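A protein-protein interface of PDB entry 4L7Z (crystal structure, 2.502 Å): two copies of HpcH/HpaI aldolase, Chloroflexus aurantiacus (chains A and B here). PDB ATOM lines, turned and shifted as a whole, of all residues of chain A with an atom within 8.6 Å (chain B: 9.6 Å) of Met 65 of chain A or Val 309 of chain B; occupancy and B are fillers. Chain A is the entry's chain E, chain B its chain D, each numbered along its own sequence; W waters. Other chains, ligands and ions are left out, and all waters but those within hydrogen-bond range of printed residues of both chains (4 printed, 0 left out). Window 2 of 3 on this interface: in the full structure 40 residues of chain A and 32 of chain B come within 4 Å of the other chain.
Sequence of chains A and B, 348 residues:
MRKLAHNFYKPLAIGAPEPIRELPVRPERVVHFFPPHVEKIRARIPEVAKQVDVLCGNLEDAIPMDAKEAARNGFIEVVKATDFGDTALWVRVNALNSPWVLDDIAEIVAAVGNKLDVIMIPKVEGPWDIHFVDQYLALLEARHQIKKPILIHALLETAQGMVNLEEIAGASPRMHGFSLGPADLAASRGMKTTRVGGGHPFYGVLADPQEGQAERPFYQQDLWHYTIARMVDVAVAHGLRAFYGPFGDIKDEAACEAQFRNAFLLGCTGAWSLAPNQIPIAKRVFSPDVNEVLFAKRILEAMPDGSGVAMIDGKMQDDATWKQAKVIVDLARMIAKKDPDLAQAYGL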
ATOM      1  N   HIS A  37      17.349  -8.139 -30.561  1.00  0.00           N
ATOM      2  CA  HIS A  37      18.432  -8.726 -31.344  1.00  0.00           C
ATOM      3  C   HIS A  37      17.959  -9.204 -32.717  1.00  0.00           C
ATOM      4  O   HIS A  37      18.767  -9.566 -33.572  1.00  0.00           O
ATOM      5  CB  HIS A  37      19.101  -9.870 -30.575  1.00  0.00           C
ATOM      6  CG  HIS A  37      18.202 -11.040 -30.328  1.00  0.00           C
ATOM      7  ND1 HIS A  37      17.039 -10.945 -29.595  1.00  0.00           N
ATOM      8  CD2 HIS A  37      18.302 -12.337 -30.709  1.00  0.00           C
ATOM      9  CE1 HIS A  37      16.458 -12.131 -29.540  1.00  0.00           C
ATOM     10  NE2 HIS A  37      17.204 -12.991 -30.206  1.00  0.00           N
ATOM     11  N   LEU A  59      16.009  -8.124 -22.571  1.00  0.00           N
ATOM     12  CA  LEU A  59      17.369  -8.642 -22.641  1.00  0.00           C
ATOM     13  C   LEU A  59      17.486  -9.960 -21.881  1.00  0.00           C
ATOM     14  O   LEU A  59      18.475 -10.680 -22.019  1.00  0.00           O
ATOM     15  CB  LEU A  59      18.354  -7.626 -22.058  1.00  0.00           C
ATOM     16  CG  LEU A  59      18.289  -6.198 -22.602  1.00  0.00           C
ATOM     17  CD1 LEU A  59      19.304  -5.313 -21.894  1.00  0.00           C
ATOM     18  CD2 LEU A  59      18.510  -6.181 -24.105  1.00  0.00           C
ATOM     19  N   GLU A  60      16.464 -10.271 -21.088  1.00  0.00           N
ATOM     20  CA  GLU A  60      16.523 -11.390 -20.152  1.00  0.00           C
ATOM     21  C   GLU A  60      16.038 -12.716 -20.748  1.00  0.00           C
ATOM     22  O   GLU A  60      16.734 -13.334 -21.553  1.00  0.00           O
ATOM     23  CB  GLU A  60      15.726 -11.062 -18.887  1.00  0.00           C
ATOM     24  CG  GLU A  60      16.067 -11.930 -17.686  1.00  0.00           C
ATOM     25  CD  GLU A  60      14.875 -12.152 -16.780  1.00  0.00           C
ATOM     26  OE1 GLU A  60      13.752 -11.765 -17.171  1.00  0.00           O
ATOM     27  OE2 GLU A  60      15.056 -12.716 -15.681  1.00  0.00           O
ATOM     28  N   ALA A  62      14.279 -15.804 -22.726  1.00  0.00           N
ATOM     29  CA  ALA A  62      14.137 -16.121 -24.149  1.00  0.00           C
ATOM     30  C   ALA A  62      15.134 -15.372 -25.038  1.00  0.00           C
ATOM     31  O   ALA A  62      15.016 -15.382 -26.263  1.00  0.00           O
ATOM     32  CB  ALA A  62      12.700 -15.898 -24.623  1.00  0.00           C
ATOM     33  N   ILE A  63      16.112 -14.726 -24.410  1.00  0.00           N
ATOM     34  CA  ILE A  63      17.210 -14.099 -25.132  1.00  0.00           C
ATOM     35  C   ILE A  63      18.465 -14.918 -24.874  1.00  0.00           C
ATOM     36  O   ILE A  63      18.981 -14.925 -23.759  1.00  0.00           O
ATOM     37  CB  ILE A  63      17.450 -12.650 -24.667  1.00  0.00           C
ATOM     38  CG1 ILE A  63      16.163 -11.828 -24.768  1.00  0.00           C
ATOM     39  CG2 ILE A  63      18.565 -12.008 -25.481  1.00  0.00           C
ATOM     40  CD1 ILE A  63      15.690 -11.600 -26.183  1.00  0.00           C
ATOM     41  N   PRO A  64      18.951 -15.622 -25.906  1.00  0.00           N
ATOM     42  CA  PRO A  64      20.099 -16.529 -25.788  1.00  0.00           C
ATOM     43  C   PRO A  64      21.331 -15.848 -25.201  1.00  0.00           C
ATOM     44  O   PRO A  64      21.488 -14.633 -25.334  1.00  0.00           O
ATOM     45  CB  PRO A  64      20.366 -16.939 -27.238  1.00  0.00           C
ATOM     46  CG  PRO A  64      19.051 -16.789 -27.916  1.00  0.00           C
ATOM     47  CD  PRO A  64      18.412 -15.594 -27.277  1.00  0.00           C
ATOM     48  N   MET A  65      22.193 -16.629 -24.558  1.00  0.00           N
ATOM     49  CA  MET A  65      23.390 -16.089 -23.928  1.00  0.00           C
ATOM     50  C   MET A  65      24.370 -15.540 -24.961  1.00  0.00           C
ATOM     51  O   MET A  65      25.104 -14.594 -24.679  1.00  0.00           O
ATOM     52  CB  MET A  65      24.072 -17.146 -23.054  1.00  0.00           C
ATOM     53  CG  MET A  65      23.172 -17.755 -21.996  1.00  0.00           C
ATOM     54  SD  MET A  65      24.066 -18.537 -20.636  1.00  0.00           S
ATOM     55  CE  MET A  65      24.920 -19.857 -21.499  1.00  0.00           C
ATOM     56  N   ASP A  66      24.376 -16.126 -26.157  1.00  0.00           N
ATOM     57  CA  ASP A  66      25.263 -15.660 -27.225  1.00  0.00           C
ATOM     58  C   ASP A  66      24.674 -14.460 -27.966  1.00  0.00           C
ATOM     59  O   ASP A  66      25.272 -13.959 -28.919  1.00  0.00           O
ATOM     60  CB  ASP A  66      25.589 -16.793 -28.212  1.00  0.00           C
ATOM     61  CG  ASP A  66      24.387 -17.221 -29.040  1.00  0.00           C
ATOM     62  OD1 ASP A  66      23.244 -16.882 -28.672  1.00  0.00           O
ATOM     63  OD2 ASP A  66      24.584 -17.915 -30.060  1.00  0.00           O
ATOM     64  N   ALA A  67      23.507 -14.002 -27.516  1.00  0.00           N
ATOM     65  CA  ALA A  67      22.822 -12.880 -28.153  1.00  0.00           C
ATOM     66  C   ALA A  67      22.588 -11.712 -27.198  1.00  0.00           C
ATOM     67  O   ALA A  67      21.928 -10.738 -27.558  1.00  0.00           O
ATOM     68  CB  ALA A  67      21.507 -13.338 -28.766  1.00  0.00           C
ATOM     69  N   LYS A  68      23.126 -11.817 -25.985  1.00  0.00           N
ATOM     70  CA  LYS A  68      22.955 -10.774 -24.974  1.00  0.00           C
ATOM     71  C   LYS A  68      23.536  -9.442 -25.436  1.00  0.00           C
ATOM     72  O   LYS A  68      22.872  -8.406 -25.369  1.00  0.00           O
ATOM     73  CB  LYS A  68      23.606 -11.191 -23.652  1.00  0.00           C
ATOM     74  CG  LYS A  68      22.983 -12.413 -23.000  1.00  0.00           C
ATOM     75  CD  LYS A  68      21.522 -12.178 -22.659  1.00  0.00           C
ATOM     76  CE  LYS A  68      20.967 -13.320 -21.822  1.00  0.00           C
ATOM     77  NZ  LYS A  68      19.504 -13.187 -21.585  1.00  0.00           N
ATOM     78  N   GLU A  69      24.782  -9.477 -25.899  1.00  0.00           N
ATOM     79  CA  GLU A  69      25.446  -8.281 -26.399  1.00  0.00           C
ATOM     80  C   GLU A  69      24.722  -7.745 -27.630  1.00  0.00           C
ATOM     81  O   GLU A  69      24.607  -6.534 -27.818  1.00  0.00           O
ATOM     82  CB  GLU A  69      26.909  -8.584 -26.727  1.00  0.00           C
ATOM     83  CG  GLU A  69      27.744  -7.364 -27.073  1.00  0.00           C
ATOM     84  CD  GLU A  69      29.220  -7.687 -27.198  1.00  0.00           C
ATOM     85  OE1 GLU A  69      29.585  -8.872 -27.046  1.00  0.00           O
ATOM     86  OE2 GLU A  69      30.017  -6.757 -27.444  1.00  0.00           O
ATOM     87  N   ALA A  70      24.226  -8.658 -28.460  1.00  0.00           N
ATOM     88  CA  ALA A  70      23.483  -8.287 -29.657  1.00  0.00           C
ATOM     89  C   ALA A  70      22.135  -7.670 -29.302  1.00  0.00           C
ATOM     90  O   ALA A  70      21.699  -6.708 -29.931  1.00  0.00           O
ATOM     91  CB  ALA A  70      23.294  -9.498 -30.561  1.00  0.00           C
ATOM     92  N   ALA A  71      21.476  -8.232 -28.293  1.00  0.00           N
ATOM     93  CA  ALA A  71      20.191  -7.713 -27.841  1.00  0.00           C
ATOM     94  C   ALA A  71      20.361  -6.342 -27.199  1.00  0.00           C
ATOM     95  O   ALA A  71      19.529  -5.453 -27.379  1.00  0.00           O
ATOM     96  CB  ALA A  71      19.536  -8.680 -26.871  1.00  0.00           C
ATOM     97  N   ARG A  72      21.448  -6.179 -26.450  1.00  0.00           N
ATOM     98  CA  ARG A  72      21.750  -4.908 -25.804  1.00  0.00           C
ATOM     99  C   ARG A  72      22.070  -3.838 -26.842  1.00  0.00           C
ATOM    100  O   ARG A  72      21.485  -2.754 -26.830  1.00  0.00           O
ATOM    101  CB  ARG A  72      22.922  -5.064 -24.835  1.00  0.00           C
ATOM    102  CG  ARG A  72      23.274  -3.790 -24.086  1.00  0.00           C
ATOM    103  CD  ARG A  72      24.574  -3.948 -23.319  1.00  0.00           C
ATOM    104  NE  ARG A  72      24.545  -5.103 -22.428  1.00  0.00           N
ATOM    105  CZ  ARG A  72      25.527  -5.993 -22.328  1.00  0.00           C
ATOM    106  NH1 ARG A  72      26.621  -5.862 -23.065  1.00  0.00           N
ATOM    107  NH2 ARG A  72      25.415  -7.014 -21.489  1.00  0.00           N
ATOM    108  N   ASN A  94      19.136  -7.902 -17.413  1.00  0.00           N
ATOM    109  CA  ASN A  94      19.332  -9.229 -16.843  1.00  0.00           C
ATOM    110  C   ASN A  94      19.335  -9.216 -15.316  1.00  0.00           C
ATOM    111  O   ASN A  94      19.253  -8.155 -14.697  1.00  0.00           O
ATOM    112  CB  ASN A  94      20.610  -9.873 -17.386  1.00  0.00           C
ATOM    113  CG  ASN A  94      20.456 -10.360 -18.816  1.00  0.00           C
ATOM    114  OD1 ASN A  94      19.934 -11.449 -19.059  1.00  0.00           O
ATOM    115  ND2 ASN A  94      20.912  -9.556 -19.770  1.00  0.00           N
ATOM    116  N   ASN A  97      22.542 -10.830 -10.475  1.00  0.00           N
ATOM    117  CA  ASN A  97      23.695 -11.702 -10.268  1.00  0.00           C
ATOM    118  C   ASN A  97      24.257 -12.222 -11.587  1.00  0.00           C
ATOM    119  O   ASN A  97      25.235 -12.970 -11.608  1.00  0.00           O
ATOM    120  CB  ASN A  97      23.333 -12.873  -9.354  1.00  0.00           C
ATOM    121  CG  ASN A  97      22.335 -13.821  -9.989  1.00  0.00           C
ATOM    122  OD1 ASN A  97      21.439 -13.401 -10.722  1.00  0.00           O
ATOM    123  ND2 ASN A  97      22.487 -15.112  -9.712  1.00  0.00           N
ATOM    124  N   SER A  98      23.630 -11.819 -12.688  1.00  0.00           N
ATOM    125  CA  SER A  98      24.057 -12.234 -14.018  1.00  0.00           C
ATOM    126  C   SER A  98      25.324 -11.496 -14.438  1.00  0.00           C
ATOM    127  O   SER A  98      25.594 -10.395 -13.954  1.00  0.00           O
ATOM    128  CB  SER A  98      22.948 -11.961 -15.032  1.00  0.00           C
ATOM    129  OG  SER A  98      22.736 -10.569 -15.177  1.00  0.00           O
ATOM    130  N   PRO A  99      26.110 -12.101 -15.342  1.00  0.00           N
ATOM    131  CA  PRO A  99      27.312 -11.447 -15.873  1.00  0.00           C
ATOM    132  C   PRO A  99      27.005 -10.437 -16.980  1.00  0.00           C
ATOM    133  O   PRO A  99      27.924 -10.013 -17.681  1.00  0.00           O
ATOM    134  CB  PRO A  99      28.113 -12.618 -16.447  1.00  0.00           C
ATOM    135  CG  PRO A  99      27.082 -13.616 -16.827  1.00  0.00           C
ATOM    136  CD  PRO A  99      26.009 -13.504 -15.781  1.00  0.00           C
ATOM    137  N   TRP A 100      25.740 -10.052 -17.131  1.00  0.00           N
ATOM    138  CA  TRP A 100      25.354  -9.122 -18.187  1.00  0.00           C
ATOM    139  C   TRP A 100      24.805  -7.799 -17.652  1.00  0.00           C
ATOM    140  O   TRP A 100      24.835  -6.784 -18.349  1.00  0.00           O
ATOM    141  CB  TRP A 100      24.317  -9.763 -19.117  1.00  0.00           C
ATOM    142  CG  TRP A 100      24.727 -11.095 -19.668  1.00  0.00           C
ATOM    143  CD1 TRP A 100      25.701 -11.334 -20.593  1.00  0.00           C
ATOM    144  CD2 TRP A 100      24.163 -12.371 -19.339  1.00  0.00           C
ATOM    145  NE1 TRP A 100      25.784 -12.681 -20.855  1.00  0.00           N
ATOM    146  CE2 TRP A 100      24.851 -13.339 -20.098  1.00  0.00           C
ATOM    147  CE3 TRP A 100      23.147 -12.788 -18.475  1.00  0.00           C
ATOM    148  CZ2 TRP A 100      24.555 -14.699 -20.018  1.00  0.00           C
ATOM    149  CZ3 TRP A 100      22.855 -14.138 -18.396  1.00  0.00           C
ATOM    150  CH2 TRP A 100      23.556 -15.077 -19.163  1.00  0.00           C
ATOM    151  N   ILE B 299      18.455 -29.727 -15.953  1.00  0.00           N
ATOM    152  CA  ILE B 299      19.174 -28.670 -15.250  1.00  0.00           C
ATOM    153  C   ILE B 299      20.454 -29.194 -14.608  1.00  0.00           C
ATOM    154  O   ILE B 299      21.512 -28.575 -14.718  1.00  0.00           O
ATOM    155  CB  ILE B 299      18.285 -28.000 -14.182  1.00  0.00           C
ATOM    156  CG1 ILE B 299      17.095 -27.303 -14.847  1.00  0.00           C
ATOM    157  CG2 ILE B 299      19.090 -27.009 -13.354  1.00  0.00           C
ATOM    158  CD1 ILE B 299      16.224 -26.528 -13.884  1.00  0.00           C
ATOM    159  N   ALA B 302      23.085 -29.866 -17.402  1.00  0.00           N
ATOM    160  CA  ALA B 302      23.713 -28.695 -18.001  1.00  0.00           C
ATOM    161  C   ALA B 302      24.738 -28.091 -17.048  1.00  0.00           C
ATOM    162  O   ALA B 302      25.666 -27.402 -17.473  1.00  0.00           O
ATOM    163  CB  ALA B 302      22.664 -27.665 -18.384  1.00  0.00           C
ATOM    164  N   MET B 303      24.559 -28.351 -15.756  1.00  0.00           N
ATOM    165  CA  MET B 303      25.443 -27.814 -14.729  1.00  0.00           C
ATOM    166  C   MET B 303      25.890 -28.907 -13.764  1.00  0.00           C
ATOM    167  O   MET B 303      25.186 -29.213 -12.802  1.00  0.00           O
ATOM    168  CB  MET B 303      24.733 -26.710 -13.944  1.00  0.00           C
ATOM    169  CG  MET B 303      23.944 -25.736 -14.798  1.00  0.00           C
ATOM    170  SD  MET B 303      23.041 -24.539 -13.801  1.00  0.00           S
ATOM    171  CE  MET B 303      24.396 -23.652 -13.038  1.00  0.00           C
ATOM    172  N   PRO B 304      27.068 -29.498 -14.017  1.00  0.00           N
ATOM    173  CA  PRO B 304      27.622 -30.554 -13.162  1.00  0.00           C
ATOM    174  C   PRO B 304      27.830 -30.109 -11.714  1.00  0.00           C
ATOM    175  O   PRO B 304      27.495 -30.856 -10.795  1.00  0.00           O
ATOM    176  CB  PRO B 304      28.973 -30.856 -13.817  1.00  0.00           C
ATOM    177  CG  PRO B 304      28.792 -30.469 -15.242  1.00  0.00           C
ATOM    178  CD  PRO B 304      27.897 -29.265 -15.213  1.00  0.00           C
ATOM    179  N   ASP B 305      28.371 -28.910 -11.517  1.00  0.00           N
ATOM    180  CA  ASP B 305      28.674 -28.423 -10.174  1.00  0.00           C
ATOM    181  C   ASP B 305      27.593 -27.491  -9.638  1.00  0.00           C
ATOM    182  O   ASP B 305      27.434 -27.345  -8.426  1.00  0.00           O
ATOM    183  CB  ASP B 305      30.022 -27.699 -10.156  1.00  0.00           C
ATOM    184  CG  ASP B 305      31.141 -28.529 -10.753  1.00  0.00           C
ATOM    185  OD1 ASP B 305      30.922 -29.150 -11.814  1.00  0.00           O
ATOM    186  OD2 ASP B 305      32.240 -28.559 -10.159  1.00  0.00           O
ATOM    187  N   GLY B 306      26.851 -26.865 -10.544  1.00  0.00           N
ATOM    188  CA  GLY B 306      25.915 -25.824 -10.167  1.00  0.00           C
ATOM    189  C   GLY B 306      26.628 -24.492 -10.245  1.00  0.00           C
ATOM    190  O   GLY B 306      26.086 -23.451  -9.867  1.00  0.00           O
ATOM    191  N   SER B 307      27.857 -24.537 -10.748  1.00  0.00           N
ATOM    192  CA  SER B 307      28.679 -23.345 -10.909  1.00  0.00           C
ATOM    193  C   SER B 307      28.648 -22.874 -12.356  1.00  0.00           C
ATOM    194  O   SER B 307      28.323 -23.642 -13.262  1.00  0.00           O
ATOM    195  CB  SER B 307      30.117 -23.629 -10.481  1.00  0.00           C
ATOM    196  OG  SER B 307      30.680 -24.679 -11.248  1.00  0.00           O
ATOM    197  N   GLY B 308      28.984 -21.608 -12.571  1.00  0.00           N
ATOM    198  CA  GLY B 308      28.953 -21.034 -13.902  1.00  0.00           C
ATOM    199  C   GLY B 308      27.551 -20.606 -14.285  1.00  0.00           C
ATOM    200  O   GLY B 308      26.619 -20.715 -13.488  1.00  0.00           O
ATOM    201  N   VAL B 309      27.398 -20.115 -15.509  1.00  0.00           N
ATOM    202  CA  VAL B 309      26.096 -19.664 -15.979  1.00  0.00           C
ATOM    203  C   VAL B 309      25.574 -20.555 -17.103  1.00  0.00           C
ATOM    204  O   VAL B 309      26.309 -20.908 -18.026  1.00  0.00           O
ATOM    205  CB  VAL B 309      26.127 -18.177 -16.423  1.00  0.00           C
ATOM    206  CG1 VAL B 309      27.187 -17.951 -17.490  1.00  0.00           C
ATOM    207  CG2 VAL B 309      24.755 -17.727 -16.909  1.00  0.00           C
ATOM    208  N   ALA B 310      24.305 -20.935 -17.006  1.00  0.00           N
ATOM    209  CA  ALA B 310      23.676 -21.772 -18.017  1.00  0.00           C
ATOM    210  C   ALA B 310      22.266 -21.280 -18.312  1.00  0.00           C
ATOM    211  O   ALA B 310      21.630 -20.655 -17.465  1.00  0.00           O
ATOM    212  CB  ALA B 310      23.650 -23.224 -17.562  1.00  0.00           C
ATOM    213  N   MET B 311      21.784 -21.559 -19.518  1.00  0.00           N
ATOM    214  CA  MET B 311      20.429 -21.182 -19.898  1.00  0.00           C
ATOM    215  C   MET B 311      19.663 -22.355 -20.499  1.00  0.00           C
ATOM    216  O   MET B 311      20.111 -22.977 -21.463  1.00  0.00           O
ATOM    217  CB  MET B 311      20.440 -20.000 -20.870  1.00  0.00           C
ATOM    218  CG  MET B 311      19.070 -19.657 -21.430  1.00  0.00           C
ATOM    219  SD  MET B 311      19.022 -18.056 -22.255  1.00  0.00           S
ATOM    220  CE  MET B 311      19.254 -16.959 -20.858  1.00  0.00           C
ATOM    221  N   ILE B 312      18.507 -22.654 -19.916  1.00  0.00           N
ATOM    222  CA  ILE B 312      17.667 -23.745 -20.391  1.00  0.00           C
ATOM    223  C   ILE B 312      16.255 -23.245 -20.673  1.00  0.00           C
ATOM    224  O   ILE B 312      15.622 -22.638 -19.808  1.00  0.00           O
ATOM    225  CB  ILE B 312      17.624 -24.899 -19.378  1.00  0.00           C
ATOM    226  CG1 ILE B 312      19.043 -25.387 -19.079  1.00  0.00           C
ATOM    227  CG2 ILE B 312      16.763 -26.038 -19.905  1.00  0.00           C
ATOM    228  CD1 ILE B 312      19.101 -26.545 -18.124  1.00  0.00           C
ATOM    229  N   ASP B 313      15.781 -23.500 -21.891  1.00  0.00           N
ATOM    230  CA  ASP B 313      14.486 -23.009 -22.358  1.00  0.00           C
ATOM    231  C   ASP B 313      14.372 -21.489 -22.250  1.00  0.00           C
ATOM    232  O   ASP B 313      13.300 -20.953 -21.960  1.00  0.00           O
ATOM    233  CB  ASP B 313      13.332 -23.701 -21.622  1.00  0.00           C
ATOM    234  CG  ASP B 313      13.179 -25.157 -22.013  1.00  0.00           C
ATOM    235  OD1 ASP B 313      13.734 -25.555 -23.059  1.00  0.00           O
ATOM    236  OD2 ASP B 313      12.493 -25.900 -21.280  1.00  0.00           O
ATOM    237  N   GLY B 314      15.488 -20.803 -22.481  1.00  0.00           N
ATOM    238  CA  GLY B 314      15.512 -19.353 -22.458  1.00  0.00           C
ATOM    239  C   GLY B 314      15.568 -18.770 -21.060  1.00  0.00           C
ATOM    240  O   GLY B 314      15.355 -17.572 -20.873  1.00  0.00           O
ATOM    241  N   LYS B 315      15.858 -19.613 -20.074  1.00  0.00           N
ATOM    242  CA  LYS B 315      15.885 -19.171 -18.685  1.00  0.00           C
ATOM    243  C   LYS B 315      17.274 -19.316 -18.079  1.00  0.00           C
ATOM    244  O   LYS B 315      17.846 -20.405 -18.077  1.00  0.00           O
ATOM    245  CB  LYS B 315      14.875 -19.965 -17.856  1.00  0.00           C
ATOM    246  CG  LYS B 315      14.666 -19.413 -16.461  1.00  0.00           C
ATOM    247  CD  LYS B 315      14.086 -18.014 -16.524  1.00  0.00           C
ATOM    248  CE  LYS B 315      14.184 -17.311 -15.185  1.00  0.00           C
ATOM    249  NZ  LYS B 315      13.523 -15.979 -15.226  1.00  0.00           N
ATOM    250  N   MET B 316      17.813 -18.217 -17.560  1.00  0.00           N
ATOM    251  CA  MET B 316      19.129 -18.247 -16.933  1.00  0.00           C
ATOM    252  C   MET B 316      19.094 -19.083 -15.663  1.00  0.00           C
ATOM    253  O   MET B 316      18.142 -19.012 -14.885  1.00  0.00           O
ATOM    254  CB  MET B 316      19.631 -16.838 -16.609  1.00  0.00           C
ATOM    255  CG  MET B 316      21.085 -16.807 -16.149  1.00  0.00           C
ATOM    256  SD  MET B 316      21.551 -15.297 -15.281  1.00  0.00           S
ATOM    257  CE  MET B 316      20.631 -15.485 -13.755  1.00  0.00           C
ATOM    258  N   GLN B 317      20.141 -19.872 -15.459  1.00  0.00           N
ATOM    259  CA  GLN B 317      20.243 -20.713 -14.279  1.00  0.00           C
ATOM    260  C   GLN B 317      21.311 -20.176 -13.333  1.00  0.00           C
ATOM    261  O   GLN B 317      22.198 -19.420 -13.741  1.00  0.00           O
ATOM    262  CB  GLN B 317      20.572 -22.148 -14.684  1.00  0.00           C
ATOM    263  CG  GLN B 317      19.550 -22.771 -15.621  1.00  0.00           C
ATOM    264  CD  GLN B 317      18.196 -22.955 -14.968  1.00  0.00           C
ATOM    265  OE1 GLN B 317      18.083 -23.577 -13.911  1.00  0.00           O
ATOM    266  NE2 GLN B 317      17.161 -22.408 -15.591  1.00  0.00           N
ATOM    267  N   ASP B 318      21.211 -20.563 -12.065  1.00  0.00           N
ATOM    268  CA  ASP B 318      22.210 -20.193 -11.070  1.00  0.00           C
ATOM    269  C   ASP B 318      22.230 -21.188  -9.913  1.00  0.00           C
ATOM    270  O   ASP B 318      21.746 -22.314 -10.042  1.00  0.00           O
ATOM    271  CB  ASP B 318      21.982 -18.762 -10.562  1.00  0.00           C
ATOM    272  CG  ASP B 318      20.558 -18.520 -10.085  1.00  0.00           C
ATOM    273  OD1 ASP B 318      19.836 -19.496  -9.799  1.00  0.00           O
ATOM    274  OD2 ASP B 318      20.161 -17.339  -9.983  1.00  0.00           O
ATOM    275  N   ASP B 319      22.783 -20.764  -8.782  1.00  0.00           N
ATOM    276  CA  ASP B 319      22.922 -21.640  -7.628  1.00  0.00           C
ATOM    277  C   ASP B 319      21.568 -21.959  -6.998  1.00  0.00           C
ATOM    278  O   ASP B 319      21.356 -23.061  -6.494  1.00  0.00           O
ATOM    279  CB  ASP B 319      23.860 -21.009  -6.599  1.00  0.00           C
ATOM    280  CG  ASP B 319      24.563 -22.043  -5.744  1.00  0.00           C
ATOM    281  OD1 ASP B 319      24.213 -22.171  -4.551  1.00  0.00           O
ATOM    282  OD2 ASP B 319      25.466 -22.733  -6.267  1.00  0.00           O
ATOM    283  N   THR B 321      18.406 -22.057  -8.522  1.00  0.00           N
ATOM    284  CA  THR B 321      17.622 -22.966  -9.351  1.00  0.00           C
ATOM    285  C   THR B 321      18.260 -24.351  -9.421  1.00  0.00           C
ATOM    286  O   THR B 321      17.571 -25.352  -9.615  1.00  0.00           O
ATOM    287  CB  THR B 321      17.442 -22.416 -10.780  1.00  0.00           C
ATOM    288  OG1 THR B 321      18.711 -22.376 -11.442  1.00  0.00           O
ATOM    289  CG2 THR B 321      16.847 -21.016 -10.742  1.00  0.00           C
HETATM  290  O   HOH W   1      12.200 -13.285 -15.444  1.00  0.00           O
HETATM  291  O   HOH W   2      19.744 -13.169 -16.044  1.00  0.00           O
HETATM  292  O   HOH W   3      21.446 -19.406 -24.780  1.00  0.00           O
HETATM  293  O   HOH W   4      14.346 -13.952 -13.033  1.00  0.00           O
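The backbone carbonyl oxygen (O) of Ile 63 of chain A lies close to the side-chain sulfur (SD) of Met 311 of chain B, 3.5 Å away. The side-chain carboxylate (OE2) of Glu 60 of chain A is in salt-bridge range of the side-chain amino group (NZ) of Lys 315 of chain B. OD2 of Asp 318 of chain B is in hydrogen-bond range of ND2 of Asn 97 of chain A (3.2 Å). The backbone carbonyl oxygen (O) of Gly 314 of chain B is in hydrogen-bond range of the backbone NH (N) of Ala 62 of chain A (2.8 Å).
The side-chain amino group (NZ) of Lys 68 of chain A lies within hydrogen-bond range of the backbone carbonyl oxygen (O) of Glu 60 of chain A (2.8 Å). The side-chain hydroxyl of Thr 321 of chain B lies within hydrogen-bond range of the backbone NH of Asp 318 of chain B (3.2 Å). The guanidinium group of Arg 72 of chain A lies within hydrogen-bond range of the backbone carbonyl oxygen of Trp 100 of chain A (3.2 Å). The backbone carbonyl oxygen (O) of Leu 59 of chain A is in hydrogen-bond range of the side-chain amino group (NZ) of Lys 68 of chain A (2.7 Å). The backbone carbonyl oxygen (O) of Lys 315 of chain B is in hydrogen-bond range of the side-chain amide nitrogen (NE2) of Gln 317 of chain B (3.3 Å). The side-chain amide oxygen of Asn 94 of chain A is in hydrogen-bond range of the side-chain amino group of Lys 68 of chain A (3.1 Å).
Among the printed residues, merely in contact across the chains: Pro 64 of chain A with Met 311 of chain B (3.997 Å), Met 65 of chain A with Val 309 of chain B (3.9 Å), Met 65 of chain A with Met 311 of chain B (3.7 Å), Lys 68 of chain A with Met 311 of chain B (3.8 Å), Asn 97 of chain A with Met 316 of chain B (3.8 Å), Ser 98 of chain A with Met 316 of chain B (3.6 Å), Trp 100 of chain A with Val 309 of chain B (3.7 Å) and Trp 100 of chain A with Met 316 of chain B (3.6 Å).
Met 65 of chain A touches two residues of chain B. Of chain A, only Met 65 (3.9 Å) and Trp 100 (3.7 Å) come within 4 Å of Val 309 of chain B. Printed residues of chain A within 4 Å of Met 316 of chain B: Asn 97 (3.8 Å), Ser 98 (3.6 Å) and Trp 100 (3.6 Å). Of the printed residues of chain B, Glu 60 of chain A touches Lys 315 (3.6 Å). Of the printed residues of chain A, Gly 314 of chain B touches Ala 62 (2.8 Å). Arg 72 of chain A touches none of the printed residues of chain B. The nearest residue of chain B that does not touch Met 65 of chain A is Ala 310 of chain B (4.02 Å). The nearest printed residue of chain A that does not touch Gly 314 of chain B is Glu 60 of chain A (4.5 Å).
Printed residues of chain A that touch a printed residue of chain B: Glu 60, Ala 62, Ile 63, Pro 64, Met 65, Lys 68, Asn 97, Ser 98 and Trp 100. Hydrophobic or aromatic side chains of chain A within 4 Å of the printed part of chain B: Met 65 and Trp 100. Hydrophobic or aromatic side chains of chain B within 4 Å of the printed part of chain A: Val 309, Met 311 and Met 316.
No position is printed for both chains. Of the 12 pairs that touch across the chains among the printed residues, none has its exchanged pair printed and touching as well.
Water W1 lies within hydrogen-bond range of the side-chain carboxylate (OE1) of Glu 60 of chain A (2.8 Å) and the side-chain amino group (NZ) of Lys 315 of chain B (3.0 Å). Water W3 bridges N of Met 65 of chain A (2.9 Å) and SD of Met 311 of chain B (3.8 Å). Water W2 bridges the side-chain sulfur of Met 316 of chain B (2.9 Å) and the side-chain amide oxygen of Asn 94 of chain A (3.5 Å). Water W4 bridges OE2 of Glu 60 of chain A and NZ of Lys 315 of chain B.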
